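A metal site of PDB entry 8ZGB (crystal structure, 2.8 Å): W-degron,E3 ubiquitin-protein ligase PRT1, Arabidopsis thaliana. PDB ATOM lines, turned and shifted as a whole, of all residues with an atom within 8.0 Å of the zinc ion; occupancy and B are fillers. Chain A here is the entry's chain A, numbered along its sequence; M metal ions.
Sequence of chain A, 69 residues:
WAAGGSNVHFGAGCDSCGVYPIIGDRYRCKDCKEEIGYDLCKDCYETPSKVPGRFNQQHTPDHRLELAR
SG of Cys 29 lies close to O of Arg 64. The backbone carbonyl oxygen (O) of Gln 58 sits close to the side-chain sulfur (SG) of Cys 32, at 3.3 Å. The backbone NH (N) of Asp 31 sits close to the side-chain sulfur (SG) of Cys 29. O of Tyr 38 sits at hydrogen-bond distance from N of Cys 29. The side-chain hydroxyl (OG1) of Thr 60 lies close to a ring nitrogen (NE2) of His 63, at 3.2 Å. N of His 59 sits at hydrogen-bond distance from O of Pro 52 (3.2 Å).
Four residues have an atom within 4 Å of the zinc ion: Cys 29, Cys 32, His 59 and His 63.
The zinc ion is bound by a ring nitrogen (ND1) of His 59 (2.0 Å), a ring nitrogen (ND1) of His 63 (2.0 Å), the side-chain sulfur (SG) of Cys 32 (2.3 Å) and the side-chain sulfur (SG) of Cys 29 (2.4 Å).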
ATOM      1  N   ARG A  28      10.592 -26.169  23.242  1.00  0.00           N
ATOM      2  CA  ARG A  28      10.954 -27.057  22.155  1.00  0.00           C
ATOM      3  C   ARG A  28      10.942 -26.238  20.869  1.00  0.00           C
ATOM      4  O   ARG A  28      10.001 -25.475  20.625  1.00  0.00           O
ATOM      5  CB  ARG A  28       9.971 -28.233  22.108  1.00  0.00           C
ATOM      6  CG  ARG A  28      10.106 -29.168  20.918  1.00  0.00           C
ATOM      7  CD  ARG A  28       9.275 -30.444  21.167  1.00  0.00           C
ATOM      8  NE  ARG A  28       7.934 -30.163  21.683  1.00  0.00           N
ATOM      9  CZ  ARG A  28       7.071 -31.102  22.087  1.00  0.00           C
ATOM     10  NH1 ARG A  28       5.874 -30.751  22.567  1.00  0.00           N
ATOM     11  NH2 ARG A  28       7.408 -32.387  22.028  1.00  0.00           N
ATOM     12  N   CYS A  29      12.003 -26.378  20.076  1.00  0.00           N
ATOM     13  CA  CYS A  29      12.096 -25.691  18.809  1.00  0.00           C
ATOM     14  C   CYS A  29      11.252 -26.404  17.768  1.00  0.00           C
ATOM     15  O   CYS A  29      11.308 -27.634  17.649  1.00  0.00           O
ATOM     16  CB  CYS A  29      13.551 -25.606  18.353  1.00  0.00           C
ATOM     17  SG  CYS A  29      13.733 -24.958  16.693  1.00  0.00           S
ATOM     18  N   LYS A  30      10.456 -25.639  17.017  1.00  0.00           N
ATOM     19  CA  LYS A  30       9.638 -26.190  15.952  1.00  0.00           C
ATOM     20  C   LYS A  30      10.307 -26.039  14.593  1.00  0.00           C
ATOM     21  O   LYS A  30       9.754 -26.493  13.589  1.00  0.00           O
ATOM     22  CB  LYS A  30       8.259 -25.511  15.933  1.00  0.00           C
ATOM     23  CG  LYS A  30       7.197 -26.231  15.077  1.00  0.00           C
ATOM     24  CD  LYS A  30       7.047 -27.702  15.421  1.00  0.00           C
ATOM     25  CE  LYS A  30       6.447 -28.490  14.244  1.00  0.00           C
ATOM     26  NZ  LYS A  30       7.271 -28.361  13.007  1.00  0.00           N
ATOM     27  N   ASP A  31      11.488 -25.414  14.545  1.00  0.00           N
ATOM     28  CA  ASP A  31      12.217 -25.189  13.297  1.00  0.00           C
ATOM     29  C   ASP A  31      13.340 -26.195  13.099  1.00  0.00           C
ATOM     30  O   ASP A  31      13.535 -26.685  11.990  1.00  0.00           O
ATOM     31  CB  ASP A  31      12.773 -23.765  13.257  1.00  0.00           C
ATOM     32  CG  ASP A  31      11.673 -22.722  13.111  1.00  0.00           C
ATOM     33  OD1 ASP A  31      10.482 -23.104  13.034  1.00  0.00           O
ATOM     34  OD2 ASP A  31      11.995 -21.520  13.077  1.00  0.00           O
ATOM     35  N   CYS A  32      14.076 -26.523  14.167  1.00  0.00           N
ATOM     36  CA  CYS A  32      15.068 -27.586  14.079  1.00  0.00           C
ATOM     37  C   CYS A  32      14.344 -28.884  13.758  1.00  0.00           C
ATOM     38  O   CYS A  32      13.600 -29.411  14.598  1.00  0.00           O
ATOM     39  CB  CYS A  32      15.869 -27.730  15.367  1.00  0.00           C
ATOM     40  SG  CYS A  32      17.276 -26.608  15.518  1.00  0.00           S
ATOM     41  N   LYS A  33      14.536 -29.411  12.556  1.00  0.00           N
ATOM     42  CA  LYS A  33      13.832 -30.612  12.126  1.00  0.00           C
ATOM     43  C   LYS A  33      14.665 -31.885  12.307  1.00  0.00           C
ATOM     44  O   LYS A  33      14.171 -32.980  12.018  1.00  0.00           O
ATOM     45  CB  LYS A  33      13.396 -30.479  10.665  1.00  0.00           C
ATOM     46  CG  LYS A  33      11.933 -30.112  10.506  1.00  0.00           C
ATOM     47  CD  LYS A  33      11.619 -28.726  11.049  1.00  0.00           C
ATOM     48  CE  LYS A  33      10.123 -28.427  10.924  1.00  0.00           C
ATOM     49  NZ  LYS A  33       9.817 -26.965  11.103  1.00  0.00           N
ATOM     50  N   GLU A  34      15.907 -31.757  12.751  1.00  0.00           N
ATOM     51  CA  GLU A  34      16.693 -32.930  13.087  1.00  0.00           C
ATOM     52  C   GLU A  34      15.903 -33.819  14.039  1.00  0.00           C
ATOM     53  O   GLU A  34      15.147 -33.344  14.881  1.00  0.00           O
ATOM     54  CB  GLU A  34      18.029 -32.510  13.724  1.00  0.00           C
ATOM     55  CG  GLU A  34      19.005 -31.809  12.781  1.00  0.00           C
ATOM     56  CD  GLU A  34      18.748 -30.314  12.660  1.00  0.00           C
ATOM     57  OE1 GLU A  34      19.577 -29.634  12.019  1.00  0.00           O
ATOM     58  OE2 GLU A  34      17.780 -29.821  13.282  1.00  0.00           O
ATOM     59  N   GLY A  37      15.563 -33.464  17.927  1.00  0.00           N
ATOM     60  CA  GLY A  37      14.875 -32.355  18.533  1.00  0.00           C
ATOM     61  C   GLY A  37      15.850 -31.337  19.105  1.00  0.00           C
ATOM     62  O   GLY A  37      17.023 -31.617  19.328  1.00  0.00           O
ATOM     63  N   TYR A  38      15.328 -30.144  19.355  1.00  0.00           N
ATOM     64  CA  TYR A  38      16.057 -29.113  20.076  1.00  0.00           C
ATOM     65  C   TYR A  38      15.159 -28.619  21.207  1.00  0.00           C
ATOM     66  O   TYR A  38      14.016 -28.196  20.977  1.00  0.00           O
ATOM     67  CB  TYR A  38      16.456 -27.979  19.134  1.00  0.00           C
ATOM     68  CG  TYR A  38      17.386 -26.939  19.736  1.00  0.00           C
ATOM     69  CD1 TYR A  38      18.764 -27.122  19.743  1.00  0.00           C
ATOM     70  CD2 TYR A  38      16.889 -25.777  20.266  1.00  0.00           C
ATOM     71  CE1 TYR A  38      19.612 -26.175  20.263  1.00  0.00           C
ATOM     72  CE2 TYR A  38      17.722 -24.804  20.794  1.00  0.00           C
ATOM     73  CZ  TYR A  38      19.083 -25.009  20.794  1.00  0.00           C
ATOM     74  OH  TYR A  38      19.906 -24.036  21.318  1.00  0.00           O
ATOM     75  N   ASP A  39      15.662 -28.696  22.424  1.00  0.00           N
ATOM     76  CA  ASP A  39      14.883 -28.315  23.591  1.00  0.00           C
ATOM     77  C   ASP A  39      15.764 -27.519  24.512  1.00  0.00           C
ATOM     78  O   ASP A  39      16.986 -27.696  24.532  1.00  0.00           O
ATOM     79  CB  ASP A  39      14.295 -29.551  24.319  1.00  0.00           C
ATOM     80  CG  ASP A  39      13.589 -30.491  23.354  1.00  0.00           C
ATOM     81  OD1 ASP A  39      12.522 -30.116  22.817  1.00  0.00           O
ATOM     82  OD2 ASP A  39      14.092 -31.604  23.141  1.00  0.00           O
ATOM     83  N   VAL A  51      23.999 -21.517  21.652  1.00  0.00           N
ATOM     84  CA  VAL A  51      24.321 -22.936  21.612  1.00  0.00           C
ATOM     85  C   VAL A  51      23.670 -23.499  20.354  1.00  0.00           C
ATOM     86  O   VAL A  51      22.443 -23.488  20.231  1.00  0.00           O
ATOM     87  CB  VAL A  51      23.853 -23.691  22.872  1.00  0.00           C
ATOM     88  CG1 VAL A  51      24.283 -22.928  24.124  1.00  0.00           C
ATOM     89  CG2 VAL A  51      22.343 -23.910  22.874  1.00  0.00           C
ATOM     90  N   PRO A  52      24.439 -23.989  19.378  1.00  0.00           N
ATOM     91  CA  PRO A  52      23.815 -24.426  18.126  1.00  0.00           C
ATOM     92  C   PRO A  52      23.142 -25.770  18.257  1.00  0.00           C
ATOM     93  O   PRO A  52      22.435 -26.205  17.335  1.00  0.00           O
ATOM     94  CB  PRO A  52      25.006 -24.497  17.169  1.00  0.00           C
ATOM     95  CG  PRO A  52      26.119 -25.005  18.075  1.00  0.00           C
ATOM     96  CD  PRO A  52      25.882 -24.322  19.427  1.00  0.00           C
ATOM     97  N   GLN A  57      22.887 -30.355  15.996  1.00  0.00           N
ATOM     98  CA  GLN A  57      21.744 -29.763  15.339  1.00  0.00           C
ATOM     99  C   GLN A  57      22.203 -28.454  14.707  1.00  0.00           C
ATOM    100  O   GLN A  57      23.309 -27.965  14.953  1.00  0.00           O
ATOM    101  CB  GLN A  57      20.627 -29.457  16.307  1.00  0.00           C
ATOM    102  CG  GLN A  57      20.093 -30.601  17.105  1.00  0.00           C
ATOM    103  CD  GLN A  57      20.773 -30.707  18.449  1.00  0.00           C
ATOM    104  OE1 GLN A  57      21.952 -30.388  18.585  1.00  0.00           O
ATOM    105  NE2 GLN A  57      20.010 -31.111  19.455  1.00  0.00           N
ATOM    106  N   GLN A  58      21.335 -27.862  13.883  1.00  0.00           N
ATOM    107  CA  GLN A  58      21.639 -26.578  13.260  1.00  0.00           C
ATOM    108  C   GLN A  58      20.497 -25.707  13.751  1.00  0.00           C
ATOM    109  O   GLN A  58      19.429 -25.676  13.137  1.00  0.00           O
ATOM    110  CB  GLN A  58      21.700 -26.692  11.770  1.00  0.00           C
ATOM    111  CG  GLN A  58      22.641 -27.801  11.312  1.00  0.00           C
ATOM    112  CD  GLN A  58      23.112 -27.616   9.880  1.00  0.00           C
ATOM    113  OE1 GLN A  58      22.794 -28.402   8.985  1.00  0.00           O
ATOM    114  NE2 GLN A  58      23.930 -26.578   9.655  1.00  0.00           N
ATOM    115  N   HIS A  59      20.734 -25.005  14.845  1.00  0.00           N
ATOM    116  CA  HIS A  59      19.713 -24.164  15.464  1.00  0.00           C
ATOM    117  C   HIS A  59      20.215 -22.739  15.344  1.00  0.00           C
ATOM    118  O   HIS A  59      21.259 -22.395  15.908  1.00  0.00           O
ATOM    119  CB  HIS A  59      19.489 -24.561  16.917  1.00  0.00           C
ATOM    120  CG  HIS A  59      18.528 -23.668  17.648  1.00  0.00           C
ATOM    121  ND1 HIS A  59      17.163 -23.848  17.584  1.00  0.00           N
ATOM    122  CD2 HIS A  59      18.732 -22.600  18.456  1.00  0.00           C
ATOM    123  CE1 HIS A  59      16.562 -22.927  18.305  1.00  0.00           C
ATOM    124  NE2 HIS A  59      17.492 -22.153  18.849  1.00  0.00           N
ATOM    125  N   THR A  60      19.490 -21.918  14.628  1.00  0.00           N
ATOM    126  CA  THR A  60      19.904 -20.559  14.413  1.00  0.00           C
ATOM    127  C   THR A  60      19.034 -19.630  15.259  1.00  0.00           C
ATOM    128  O   THR A  60      17.880 -19.961  15.560  1.00  0.00           O
ATOM    129  CB  THR A  60      19.784 -20.189  12.928  1.00  0.00           C
ATOM    130  OG1 THR A  60      18.622 -20.801  12.355  1.00  0.00           O
ATOM    131  CG2 THR A  60      21.012 -20.691  12.177  1.00  0.00           C
ATOM    132  N   PRO A  61      19.562 -18.483  15.698  1.00  0.00           N
ATOM    133  CA  PRO A  61      18.777 -17.631  16.609  1.00  0.00           C
ATOM    134  C   PRO A  61      17.411 -17.237  16.059  1.00  0.00           C
ATOM    135  O   PRO A  61      16.560 -16.814  16.846  1.00  0.00           O
ATOM    136  CB  PRO A  61      19.684 -16.406  16.808  1.00  0.00           C
ATOM    137  CG  PRO A  61      21.069 -16.910  16.538  1.00  0.00           C
ATOM    138  CD  PRO A  61      20.902 -17.937  15.431  1.00  0.00           C
ATOM    139  N   ASP A  62      17.171 -17.360  14.743  1.00  0.00           N
ATOM    140  CA  ASP A  62      15.848 -17.071  14.202  1.00  0.00           C
ATOM    141  C   ASP A  62      14.842 -18.191  14.416  1.00  0.00           C
ATOM    142  O   ASP A  62      13.653 -17.989  14.158  1.00  0.00           O
ATOM    143  CB  ASP A  62      15.954 -16.768  12.700  1.00  0.00           C
ATOM    144  CG  ASP A  62      16.406 -17.971  11.889  1.00  0.00           C
ATOM    145  OD1 ASP A  62      17.178 -18.798  12.416  1.00  0.00           O
ATOM    146  OD2 ASP A  62      15.980 -18.084  10.709  1.00  0.00           O
ATOM    147  N   HIS A  63      15.274 -19.363  14.875  1.00  0.00           N
ATOM    148  CA  HIS A  63      14.353 -20.476  15.091  1.00  0.00           C
ATOM    149  C   HIS A  63      13.317 -20.113  16.146  1.00  0.00           C
ATOM    150  O   HIS A  63      13.583 -19.359  17.088  1.00  0.00           O
ATOM    151  CB  HIS A  63      15.113 -21.744  15.499  1.00  0.00           C
ATOM    152  CG  HIS A  63      15.703 -22.496  14.347  1.00  0.00           C
ATOM    153  ND1 HIS A  63      16.088 -23.813  14.434  1.00  0.00           N
ATOM    154  CD2 HIS A  63      15.972 -22.113  13.072  1.00  0.00           C
ATOM    155  CE1 HIS A  63      16.572 -24.206  13.275  1.00  0.00           C
ATOM    156  NE2 HIS A  63      16.511 -23.195  12.433  1.00  0.00           N
ATOM    157  N   ARG A  64      12.111 -20.675  15.990  1.00  0.00           N
ATOM    158  CA  ARG A  64      10.993 -20.414  16.885  1.00  0.00           C
ATOM    159  C   ARG A  64      10.918 -21.524  17.933  1.00  0.00           C
ATOM    160  O   ARG A  64      11.224 -22.684  17.652  1.00  0.00           O
ATOM    161  CB  ARG A  64       9.681 -20.361  16.102  1.00  0.00           C
ATOM    162  CG  ARG A  64       9.691 -19.425  14.911  1.00  0.00           C
ATOM    163  CD  ARG A  64       8.336 -19.417  14.183  1.00  0.00           C
ATOM    164  NE  ARG A  64       7.251 -18.906  15.033  1.00  0.00           N
ATOM    165  CZ  ARG A  64       5.962 -18.878  14.665  1.00  0.00           C
ATOM    166  NH1 ARG A  64       5.593 -19.320  13.477  1.00  0.00           N
ATOM    167  NH2 ARG A  64       5.045 -18.403  15.503  1.00  0.00           N
ATOM    168  N   LEU A  65      10.509 -21.151  19.147  1.00  0.00           N
ATOM    169  CA  LEU A  65      10.400 -22.087  20.262  1.00  0.00           C
ATOM    170  C   LEU A  65       9.047 -21.965  20.953  1.00  0.00           C
ATOM    171  O   LEU A  65       8.564 -20.860  21.195  1.00  0.00           O
ATOM    172  CB  LEU A  65      11.520 -21.837  21.275  1.00  0.00           C
ATOM    173  CG  LEU A  65      12.960 -22.048  20.775  1.00  0.00           C
ATOM    174  CD1 LEU A  65      13.469 -20.810  20.053  1.00  0.00           C
ATOM    175  CD2 LEU A  65      13.915 -22.441  21.895  1.00  0.00           C
HETATM  176 ZN    ZN M   1      16.074 -24.777  16.209  1.00  0.00          ZN
